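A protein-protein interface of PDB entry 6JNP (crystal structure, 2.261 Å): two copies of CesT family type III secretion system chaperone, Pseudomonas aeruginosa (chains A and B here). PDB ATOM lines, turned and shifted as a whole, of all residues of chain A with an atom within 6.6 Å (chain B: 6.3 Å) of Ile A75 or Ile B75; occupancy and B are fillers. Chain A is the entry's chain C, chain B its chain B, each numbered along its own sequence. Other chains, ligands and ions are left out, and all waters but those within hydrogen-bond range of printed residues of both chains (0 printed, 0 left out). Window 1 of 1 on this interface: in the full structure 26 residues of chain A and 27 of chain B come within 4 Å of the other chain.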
ATOM      1  N   GLN A  64     -13.680  17.251  12.665  1.00  0.00           N
ATOM      2  CA  GLN A  64     -12.547  16.341  12.797  1.00  0.00           C
ATOM      3  C   GLN A  64     -12.711  15.418  13.999  1.00  0.00           C
ATOM      4  O   GLN A  64     -12.303  14.251  13.953  1.00  0.00           O
ATOM      5  CB  GLN A  64     -11.246  17.138  12.910  1.00  0.00           C
ATOM      6  CG  GLN A  64     -10.011  16.290  13.188  1.00  0.00           C
ATOM      7  CD  GLN A  64      -9.643  15.392  12.024  1.00  0.00           C
ATOM      8  OE1 GLN A  64      -9.744  15.790  10.863  1.00  0.00           O
ATOM      9  NE2 GLN A  64      -9.215  14.172  12.328  1.00  0.00           N
ATOM     10  N   ASN A  65     -13.303  15.918  15.081  1.00  0.00           N
ATOM     11  CA  ASN A  65     -13.466  15.143  16.302  1.00  0.00           C
ATOM     12  C   ASN A  65     -14.784  14.378  16.340  1.00  0.00           C
ATOM     13  O   ASN A  65     -15.243  13.999  17.424  1.00  0.00           O
ATOM     14  CB  ASN A  65     -13.335  16.057  17.520  1.00  0.00           C
ATOM     15  CG  ASN A  65     -11.985  16.742  17.580  1.00  0.00           C
ATOM     16  OD1 ASN A  65     -10.979  16.194  17.126  1.00  0.00           O
ATOM     17  ND2 ASN A  65     -11.956  17.950  18.128  1.00  0.00           N
ATOM     18  N   LEU A  66     -15.396  14.140  15.187  1.00  0.00           N
ATOM     19  CA  LEU A  66     -16.551  13.263  15.083  1.00  0.00           C
ATOM     20  C   LEU A  66     -16.096  11.897  14.587  1.00  0.00           C
ATOM     21  O   LEU A  66     -15.241  11.803  13.701  1.00  0.00           O
ATOM     22  CB  LEU A  66     -17.600  13.849  14.137  1.00  0.00           C
ATOM     23  CG  LEU A  66     -18.913  13.077  14.020  1.00  0.00           C
ATOM     24  CD1 LEU A  66     -19.580  12.938  15.380  1.00  0.00           C
ATOM     25  CD2 LEU A  66     -19.832  13.774  13.046  1.00  0.00           C
ATOM     26  N   PHE A  67     -16.662  10.844  15.171  1.00  0.00           N
ATOM     27  CA  PHE A  67     -16.276   9.485  14.818  1.00  0.00           C
ATOM     28  C   PHE A  67     -16.541   9.210  13.339  1.00  0.00           C
ATOM     29  O   PHE A  67     -17.366   9.864  12.694  1.00  0.00           O
ATOM     30  CB  PHE A  67     -17.037   8.476  15.679  1.00  0.00           C
ATOM     31  CG  PHE A  67     -18.534   8.611  15.593  1.00  0.00           C
ATOM     32  CD1 PHE A  67     -19.252   7.937  14.618  1.00  0.00           C
ATOM     33  CD2 PHE A  67     -19.224   9.418  16.486  1.00  0.00           C
ATOM     34  CE1 PHE A  67     -20.626   8.063  14.534  1.00  0.00           C
ATOM     35  CE2 PHE A  67     -20.599   9.547  16.408  1.00  0.00           C
ATOM     36  CZ  PHE A  67     -21.301   8.870  15.431  1.00  0.00           C
ATOM     37  N   CYS A  72      -8.809   4.923  13.811  1.00  0.00           N
ATOM     38  CA  CYS A  72      -7.564   5.676  13.829  1.00  0.00           C
ATOM     39  C   CYS A  72      -7.737   7.119  13.383  1.00  0.00           C
ATOM     40  O   CYS A  72      -6.739   7.840  13.289  1.00  0.00           O
ATOM     41  CB  CYS A  72      -6.520   4.992  12.943  1.00  0.00           C
ATOM     42  SG  CYS A  72      -5.970   3.393  13.561  1.00  0.00           S
ATOM     43  N   LYS A  73      -8.961   7.551  13.097  1.00  0.00           N
ATOM     44  CA  LYS A  73      -9.203   8.942  12.748  1.00  0.00           C
ATOM     45  C   LYS A  73      -8.720   9.832  13.886  1.00  0.00           C
ATOM     46  O   LYS A  73      -9.209   9.697  15.017  1.00  0.00           O
ATOM     47  CB  LYS A  73     -10.682   9.195  12.474  1.00  0.00           C
ATOM     48  CG  LYS A  73     -10.980  10.632  12.072  1.00  0.00           C
ATOM     49  CD  LYS A  73     -12.469  10.868  11.901  1.00  0.00           C
ATOM     50  CE  LYS A  73     -12.747  12.294  11.463  1.00  0.00           C
ATOM     51  NZ  LYS A  73     -14.205  12.556  11.320  1.00  0.00           N
ATOM     52  N   PRO A  74      -7.767  10.725  13.646  1.00  0.00           N
ATOM     53  CA  PRO A  74      -7.182  11.489  14.751  1.00  0.00           C
ATOM     54  C   PRO A  74      -8.167  12.471  15.365  1.00  0.00           C
ATOM     55  O   PRO A  74      -9.055  13.011  14.700  1.00  0.00           O
ATOM     56  CB  PRO A  74      -6.006  12.219  14.092  1.00  0.00           C
ATOM     57  CG  PRO A  74      -5.702  11.416  12.864  1.00  0.00           C
ATOM     58  CD  PRO A  74      -7.033  10.928  12.387  1.00  0.00           C
ATOM     59  N   ILE A  75      -7.995  12.682  16.665  1.00  0.00           N
ATOM     60  CA  ILE A  75      -8.755  13.646  17.450  1.00  0.00           C
ATOM     61  C   ILE A  75      -7.891  14.882  17.645  1.00  0.00           C
ATOM     62  O   ILE A  75      -6.685  14.775  17.906  1.00  0.00           O
ATOM     63  CB  ILE A  75      -9.171  13.046  18.807  1.00  0.00           C
ATOM     64  CG1 ILE A  75      -9.883  11.707  18.607  1.00  0.00           C
ATOM     65  CG2 ILE A  75     -10.037  14.027  19.587  1.00  0.00           C
ATOM     66  CD1 ILE A  75     -11.151  11.803  17.801  1.00  0.00           C
ATOM     67  N   LEU A  76      -8.504  16.056  17.523  1.00  0.00           N
ATOM     68  CA  LEU A  76      -7.815  17.337  17.663  1.00  0.00           C
ATOM     69  C   LEU A  76      -8.221  17.969  18.991  1.00  0.00           C
ATOM     70  O   LEU A  76      -9.299  18.558  19.104  1.00  0.00           O
ATOM     71  CB  LEU A  76      -8.139  18.257  16.489  1.00  0.00           C
ATOM     72  CG  LEU A  76      -7.476  19.636  16.504  1.00  0.00           C
ATOM     73  CD1 LEU A  76      -5.961  19.500  16.531  1.00  0.00           C
ATOM     74  CD2 LEU A  76      -7.927  20.459  15.306  1.00  0.00           C
ATOM     75  N   GLY A  77      -7.353  17.843  19.994  1.00  0.00           N
ATOM     76  CA  GLY A  77      -7.552  18.470  21.278  1.00  0.00           C
ATOM     77  C   GLY A  77      -6.600  19.628  21.503  1.00  0.00           C
ATOM     78  O   GLY A  77      -5.873  20.062  20.608  1.00  0.00           O
ATOM     79  N   LEU A  86      -3.209  19.572  19.645  1.00  0.00           N
ATOM     80  CA  LEU A  86      -2.604  18.248  19.649  1.00  0.00           C
ATOM     81  C   LEU A  86      -3.496  17.299  18.866  1.00  0.00           C
ATOM     82  O   LEU A  86      -4.664  17.106  19.219  1.00  0.00           O
ATOM     83  CB  LEU A  86      -2.416  17.737  21.079  1.00  0.00           C
ATOM     84  CG  LEU A  86      -1.233  18.286  21.869  1.00  0.00           C
ATOM     85  CD1 LEU A  86      -1.566  18.344  23.346  1.00  0.00           C
ATOM     86  CD2 LEU A  86      -0.016  17.413  21.634  1.00  0.00           C
ATOM     87  N   LEU A  87      -2.949  16.712  17.809  1.00  0.00           N
ATOM     88  CA  LEU A  87      -3.632  15.663  17.074  1.00  0.00           C
ATOM     89  C   LEU A  87      -3.174  14.316  17.616  1.00  0.00           C
ATOM     90  O   LEU A  87      -1.985  14.118  17.867  1.00  0.00           O
ATOM     91  CB  LEU A  87      -3.321  15.779  15.583  1.00  0.00           C
ATOM     92  CG  LEU A  87      -4.412  15.376  14.601  1.00  0.00           C
ATOM     93  CD1 LEU A  87      -5.717  16.063  14.937  1.00  0.00           C
ATOM     94  CD2 LEU A  87      -3.969  15.760  13.220  1.00  0.00           C
ATOM     95  N   TRP A  88      -4.116  13.399  17.821  1.00  0.00           N
ATOM     96  CA  TRP A  88      -3.748  12.146  18.472  1.00  0.00           C
ATOM     97  C   TRP A  88      -4.732  11.043  18.119  1.00  0.00           C
ATOM     98  O   TRP A  88      -5.932  11.284  18.011  1.00  0.00           O
ATOM     99  CB  TRP A  88      -3.692  12.313  19.995  1.00  0.00           C
ATOM    100  CG  TRP A  88      -5.027  12.612  20.604  1.00  0.00           C
ATOM    101  CD1 TRP A  88      -5.575  13.843  20.814  1.00  0.00           C
ATOM    102  CD2 TRP A  88      -5.986  11.660  21.077  1.00  0.00           C
ATOM    103  NE1 TRP A  88      -6.815  13.716  21.391  1.00  0.00           N
ATOM    104  CE2 TRP A  88      -7.091  12.385  21.563  1.00  0.00           C
ATOM    105  CE3 TRP A  88      -6.017  10.263  21.138  1.00  0.00           C
ATOM    106  CZ2 TRP A  88      -8.215  11.764  22.102  1.00  0.00           C
ATOM    107  CZ3 TRP A  88      -7.132   9.647  21.673  1.00  0.00           C
ATOM    108  CH2 TRP A  88      -8.217  10.397  22.148  1.00  0.00           C
ATOM    109  N   ASN A  89      -4.214   9.827  17.973  1.00  0.00           N
ATOM    110  CA  ASN A  89      -5.047   8.640  17.839  1.00  0.00           C
ATOM    111  C   ASN A  89      -4.462   7.531  18.705  1.00  0.00           C
ATOM    112  O   ASN A  89      -3.360   7.653  19.247  1.00  0.00           O
ATOM    113  CB  ASN A  89      -5.178   8.197  16.375  1.00  0.00           C
ATOM    114  CG  ASN A  89      -3.839   8.042  15.687  1.00  0.00           C
ATOM    115  OD1 ASN A  89      -2.795   7.958  16.338  1.00  0.00           O
ATOM    116  ND2 ASN A  89      -3.862   7.998  14.360  1.00  0.00           N
ATOM    117  N   LEU A 108      -2.488   9.752  11.431  1.00  0.00           N
ATOM    118  CA  LEU A 108      -2.011  10.893  12.205  1.00  0.00           C
ATOM    119  C   LEU A 108      -1.323  11.916  11.306  1.00  0.00           C
ATOM    120  O   LEU A 108      -1.635  13.112  11.352  1.00  0.00           O
ATOM    121  CB  LEU A 108      -1.067  10.426  13.311  1.00  0.00           C
ATOM    122  CG  LEU A 108      -0.707  11.513  14.327  1.00  0.00           C
ATOM    123  CD1 LEU A 108      -1.930  11.899  15.143  1.00  0.00           C
ATOM    124  CD2 LEU A 108       0.434  11.069  15.233  1.00  0.00           C
ATOM    125  N   LEU A 115      -5.390  19.549   8.511  1.00  0.00           N
ATOM    126  CA  LEU A 115      -5.807  20.630   9.398  1.00  0.00           C
ATOM    127  C   LEU A 115      -4.728  21.703   9.482  1.00  0.00           C
ATOM    128  O   LEU A 115      -3.556  21.399   9.721  1.00  0.00           O
ATOM    129  CB  LEU A 115      -6.110  20.075  10.791  1.00  0.00           C
ATOM    130  CG  LEU A 115      -6.939  18.789  10.846  1.00  0.00           C
ATOM    131  CD1 LEU A 115      -7.106  18.321  12.283  1.00  0.00           C
ATOM    132  CD2 LEU A 115      -8.293  18.978  10.177  1.00  0.00           C
ATOM    133  N   GLN B  64     -11.827  18.472  26.538  1.00  0.00           N
ATOM    134  CA  GLN B  64     -12.515  17.195  26.403  1.00  0.00           C
ATOM    135  C   GLN B  64     -11.911  16.346  25.290  1.00  0.00           C
ATOM    136  O   GLN B  64     -11.868  15.115  25.403  1.00  0.00           O
ATOM    137  CB  GLN B  64     -14.002  17.431  26.139  1.00  0.00           C
ATOM    138  CG  GLN B  64     -14.851  16.175  26.185  1.00  0.00           C
ATOM    139  CD  GLN B  64     -14.958  15.603  27.583  1.00  0.00           C
ATOM    140  OE1 GLN B  64     -15.227  16.327  28.543  1.00  0.00           O
ATOM    141  NE2 GLN B  64     -14.740  14.299  27.708  1.00  0.00           N
ATOM    142  N   ASN B  65     -11.439  16.978  24.218  1.00  0.00           N
ATOM    143  CA  ASN B  65     -10.893  16.266  23.072  1.00  0.00           C
ATOM    144  C   ASN B  65      -9.400  15.986  23.197  1.00  0.00           C
ATOM    145  O   ASN B  65      -8.764  15.625  22.203  1.00  0.00           O
ATOM    146  CB  ASN B  65     -11.176  17.048  21.789  1.00  0.00           C
ATOM    147  CG  ASN B  65     -12.657  17.166  21.501  1.00  0.00           C
ATOM    148  OD1 ASN B  65     -13.437  16.281  21.846  1.00  0.00           O
ATOM    149  ND2 ASN B  65     -13.054  18.264  20.872  1.00  0.00           N
ATOM    150  N   LEU B  66      -8.832  16.141  24.389  1.00  0.00           N
ATOM    151  CA  LEU B  66      -7.449  15.774  24.650  1.00  0.00           C
ATOM    152  C   LEU B  66      -7.406  14.398  25.299  1.00  0.00           C
ATOM    153  O   LEU B  66      -8.215  14.090  26.180  1.00  0.00           O
ATOM    154  CB  LEU B  66      -6.767  16.805  25.552  1.00  0.00           C
ATOM    155  CG  LEU B  66      -5.273  16.592  25.797  1.00  0.00           C
ATOM    156  CD1 LEU B  66      -4.522  16.555  24.476  1.00  0.00           C
ATOM    157  CD2 LEU B  66      -4.715  17.676  26.707  1.00  0.00           C
ATOM    158  N   PRO B  71      -9.010   5.343  27.823  1.00  0.00           N
ATOM    159  CA  PRO B  71      -9.453   5.326  26.419  1.00  0.00           C
ATOM    160  C   PRO B  71     -10.934   5.611  26.251  1.00  0.00           C
ATOM    161  O   PRO B  71     -11.356   5.977  25.148  1.00  0.00           O
ATOM    162  CB  PRO B  71      -9.104   3.904  25.955  1.00  0.00           C
ATOM    163  CG  PRO B  71      -8.075   3.421  26.929  1.00  0.00           C
ATOM    164  CD  PRO B  71      -8.425   4.058  28.235  1.00  0.00           C
ATOM    165  N   CYS B  72     -11.733   5.457  27.303  1.00  0.00           N
ATOM    166  CA  CYS B  72     -13.162   5.727  27.238  1.00  0.00           C
ATOM    167  C   CYS B  72     -13.505   7.188  27.482  1.00  0.00           C
ATOM    168  O   CYS B  72     -14.693   7.519  27.550  1.00  0.00           O
ATOM    169  CB  CYS B  72     -13.912   4.856  28.248  1.00  0.00           C
ATOM    170  SG  CYS B  72     -13.939   3.108  27.820  1.00  0.00           S
ATOM    171  N   LYS B  73     -12.513   8.060  27.627  1.00  0.00           N
ATOM    172  CA  LYS B  73     -12.800   9.480  27.745  1.00  0.00           C
ATOM    173  C   LYS B  73     -13.493   9.949  26.471  1.00  0.00           C
ATOM    174  O   LYS B  73     -12.940   9.776  25.375  1.00  0.00           O
ATOM    175  CB  LYS B  73     -11.534  10.298  27.983  1.00  0.00           C
ATOM    176  CG  LYS B  73     -11.824  11.777  28.203  1.00  0.00           C
ATOM    177  CD  LYS B  73     -10.564  12.620  28.210  1.00  0.00           C
ATOM    178  CE  LYS B  73     -10.905  14.093  28.375  1.00  0.00           C
ATOM    179  NZ  LYS B  73      -9.718  14.975  28.201  1.00  0.00           N
ATOM    180  N   PRO B  74     -14.689  10.519  26.561  1.00  0.00           N
ATOM    181  CA  PRO B  74     -15.437  10.852  25.346  1.00  0.00           C
ATOM    182  C   PRO B  74     -14.824  12.019  24.591  1.00  0.00           C
ATOM    183  O   PRO B  74     -14.193  12.909  25.167  1.00  0.00           O
ATOM    184  CB  PRO B  74     -16.832  11.207  25.874  1.00  0.00           C
ATOM    185  CG  PRO B  74     -16.889  10.623  27.254  1.00  0.00           C
ATOM    186  CD  PRO B  74     -15.493  10.716  27.776  1.00  0.00           C
ATOM    187  N   ILE B  75     -15.021  11.993  23.279  1.00  0.00           N
ATOM    188  CA  ILE B  75     -14.632  13.057  22.366  1.00  0.00           C
ATOM    189  C   ILE B  75     -15.889  13.816  21.963  1.00  0.00           C
ATOM    190  O   ILE B  75     -16.952  13.216  21.750  1.00  0.00           O
ATOM    191  CB  ILE B  75     -13.907  12.487  21.130  1.00  0.00           C
ATOM    192  CG1 ILE B  75     -12.621  11.763  21.539  1.00  0.00           C
ATOM    193  CG2 ILE B  75     -13.602  13.579  20.124  1.00  0.00           C
ATOM    194  CD1 ILE B  75     -12.777  10.261  21.669  1.00  0.00           C
ATOM    195  N   LEU B  76     -15.773  15.139  21.869  1.00  0.00           N
ATOM    196  CA  LEU B  76     -16.881  16.006  21.483  1.00  0.00           C
ATOM    197  C   LEU B  76     -16.673  16.460  20.040  1.00  0.00           C
ATOM    198  O   LEU B  76     -15.781  17.268  19.759  1.00  0.00           O
ATOM    199  CB  LEU B  76     -16.979  17.201  22.430  1.00  0.00           C
ATOM    200  CG  LEU B  76     -17.959  18.323  22.077  1.00  0.00           C
ATOM    201  CD1 LEU B  76     -19.370  17.788  21.889  1.00  0.00           C
ATOM    202  CD2 LEU B  76     -17.932  19.396  23.153  1.00  0.00           C
ATOM    203  N   GLY B  77     -17.491  15.933  19.128  1.00  0.00           N
ATOM    204  CA  GLY B  77     -17.476  16.335  17.740  1.00  0.00           C
ATOM    205  C   GLY B  77     -18.803  16.956  17.336  1.00  0.00           C
ATOM    206  O   GLY B  77     -19.710  17.130  18.152  1.00  0.00           O
ATOM    207  N   LEU B  86     -22.089  15.947  19.238  1.00  0.00           N
ATOM    208  CA  LEU B  86     -22.142  14.566  19.693  1.00  0.00           C
ATOM    209  C   LEU B  86     -20.940  14.273  20.575  1.00  0.00           C
ATOM    210  O   LEU B  86     -19.794  14.511  20.175  1.00  0.00           O
ATOM    211  CB  LEU B  86     -22.174  13.603  18.505  1.00  0.00           C
ATOM    212  CG  LEU B  86     -23.272  13.897  17.483  1.00  0.00           C
ATOM    213  CD1 LEU B  86     -23.121  13.002  16.276  1.00  0.00           C
ATOM    214  CD2 LEU B  86     -24.646  13.731  18.114  1.00  0.00           C
ATOM    215  N   LEU B  87     -21.206  13.757  21.768  1.00  0.00           N
ATOM    216  CA  LEU B  87     -20.175  13.278  22.676  1.00  0.00           C
ATOM    217  C   LEU B  87     -20.147  11.758  22.570  1.00  0.00           C
ATOM    218  O   LEU B  87     -21.172  11.106  22.780  1.00  0.00           O
ATOM    219  CB  LEU B  87     -20.484  13.729  24.102  1.00  0.00           C
ATOM    220  CG  LEU B  87     -19.436  13.600  25.198  1.00  0.00           C
ATOM    221  CD1 LEU B  87     -18.297  14.585  24.984  1.00  0.00           C
ATOM    222  CD2 LEU B  87     -20.111  13.837  26.529  1.00  0.00           C
ATOM    223  N   TRP B  88     -18.988  11.193  22.229  1.00  0.00           N
ATOM    224  CA  TRP B  88     -18.930   9.783  21.868  1.00  0.00           C
ATOM    225  C   TRP B  88     -17.664   9.127  22.402  1.00  0.00           C
ATOM    226  O   TRP B  88     -16.649   9.779  22.639  1.00  0.00           O
ATOM    227  CB  TRP B  88     -18.995   9.595  20.346  1.00  0.00           C
ATOM    228  CG  TRP B  88     -17.817  10.162  19.613  1.00  0.00           C
ATOM    229  CD1 TRP B  88     -17.662  11.445  19.177  1.00  0.00           C
ATOM    230  CD2 TRP B  88     -16.631   9.459  19.221  1.00  0.00           C
ATOM    231  NE1 TRP B  88     -16.453  11.587  18.542  1.00  0.00           N
ATOM    232  CE2 TRP B  88     -15.801  10.381  18.554  1.00  0.00           C
ATOM    233  CE3 TRP B  88     -16.189   8.142  19.371  1.00  0.00           C
ATOM    234  CZ2 TRP B  88     -14.557  10.028  18.039  1.00  0.00           C
ATOM    235  CZ3 TRP B  88     -14.954   7.794  18.858  1.00  0.00           C
ATOM    236  CH2 TRP B  88     -14.152   8.733  18.201  1.00  0.00           C
ATOM    237  N   ASN B  89     -17.741   7.812  22.581  1.00  0.00           N
ATOM    238  CA  ASN B  89     -16.562   6.998  22.842  1.00  0.00           C
ATOM    239  C   ASN B  89     -16.743   5.650  22.160  1.00  0.00           C
ATOM    240  O   ASN B  89     -17.842   5.286  21.731  1.00  0.00           O
ATOM    241  CB  ASN B  89     -16.292   6.843  24.344  1.00  0.00           C
ATOM    242  CG  ASN B  89     -17.480   6.293  25.108  1.00  0.00           C
ATOM    243  OD1 ASN B  89     -18.426   5.762  24.526  1.00  0.00           O
ATOM    244  ND2 ASN B  89     -17.429   6.410  26.429  1.00  0.00           N
ATOM    245  N   ARG B  90     -15.640   4.909  22.056  1.00  0.00           N
ATOM    246  CA  ARG B  90     -15.625   3.680  21.277  1.00  0.00           C
ATOM    247  C   ARG B  90     -14.627   2.704  21.880  1.00  0.00           C
ATOM    248  O   ARG B  90     -13.588   3.105  22.414  1.00  0.00           O
ATOM    249  CB  ARG B  90     -15.281   3.972  19.811  1.00  0.00           C
ATOM    250  CG  ARG B  90     -15.197   2.750  18.917  1.00  0.00           C
ATOM    251  CD  ARG B  90     -15.523   3.114  17.484  1.00  0.00           C
ATOM    252  NE  ARG B  90     -14.664   4.176  16.973  1.00  0.00           N
ATOM    253  CZ  ARG B  90     -14.953   4.919  15.910  1.00  0.00           C
ATOM    254  NH1 ARG B  90     -16.086   4.722  15.251  1.00  0.00           N
ATOM    255  NH2 ARG B  90     -14.111   5.863  15.512  1.00  0.00           N
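N of Gly B77 lies close to O of Asn A65 (3.4 Å).
NE1 of Trp B88 sits at hydrogen-bond distance from O of Asn A65, 2.9 Å away.
The backbone NH (N) of Phe A67 lies close to the indole nitrogen (NE1) of Trp B88 (3.5 Å).
ND2 of Asn B65 lies close to ND2 of Asn A65, 3.0 Å away.
O of Asn B65 sits at hydrogen-bond distance from NE1 of Trp A88 (2.8 Å).
The backbone NH of Gly A77 sits close to the backbone carbonyl oxygen of Asn B65.
The backbone NH (N) of Ile A75 is in hydrogen-bond range of the backbone carbonyl oxygen (O) of Trp A88 (2.8 Å).
The backbone NH (N) of Ile B75 is in hydrogen-bond range of the backbone carbonyl oxygen (O) of Trp B88, at 2.8 Å.
The side-chain amino group (NZ) of Lys A73 lies within hydrogen-bond range of the backbone carbonyl oxygen (O) of Leu A66.
The side-chain amide oxygen (OD1) of Asn B65 sits at hydrogen-bond distance from the backbone NH (N) of Leu B76 (2.6 Å).
The side-chain amide oxygen of Asn A65 sits at hydrogen-bond distance from the backbone NH of Leu A76.
NZ of Lys B73 lies within hydrogen-bond range of O of Leu B66, at 2.7 Å.
Asn A65 touches Leu B76 (CB to O, 3.5 Å).
Gly B77 touches Leu A66 (CA to N, 3.96 Å).
CD1 of Leu B86 touches CD1 of Leu A66, at 3.7 Å.
Leu A66 touches Trp B88.
Arg B90 touches Phe A67 (NH1 to CB, 3.9 Å).
O of Asn B65 touches CG2 of Ile A75 (3.3 Å).
CG2 of Ile A75 touches CG2 of Ile B75, at 3.6 Å.
CD1 of Ile A75 touches CZ2 of Trp B88 (3.8 Å).
Leu A76 touches Asn B65 (O to CB, 3.6 Å).
NE1 of Trp A88 touches CA of Leu B66, 3.9 Å away.
Ile A75 touches three residues of chain B.
Printed residues of chain A within 4 Å of Ile B75: Asn A65 and Ile A75.
Printed residues of chain A within 4 Å of Gly B77: Asn A65 and Leu A66.
Of the printed residues of chain B, Trp A88 touches Asn B65 and Leu B66.
The nearest residue of chain B that does not touch Ile A75 is Leu B66 (5.4 Å).
Of the 16 printed residues of chain A, 8 touch a printed residue of chain B.
Of the 15 printed residues of chain B, 8 touch a printed residue of chain A.
Hydrophobic or aromatic side chains of chain B within 4 Å of the printed part of chain A: Leu B66, Ile B75, Leu B86 and Trp B88.
Among the printed residues, 18 pairs touch across the chains.
Among the printed residues, no Asp or Glu carboxylate lies within 4 Å of a Lys or Arg side-chain nitrogen of the other chain.
Asn A65 touches Ile B75, and with the chains exchanged Ile A75 touches Asn B65.
Asn A65 touches Leu B76, and with the chains exchanged Leu A76 touches Asn B65.
Leu A66 touches Gly B77, but with the chains exchanged Gly A77 does not touch Leu B66 (4.1 Å).
Leu A66 touches Leu B86, and with the chains exchanged Leu A86 touches Leu B66.
13 positions are printed for both chains.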
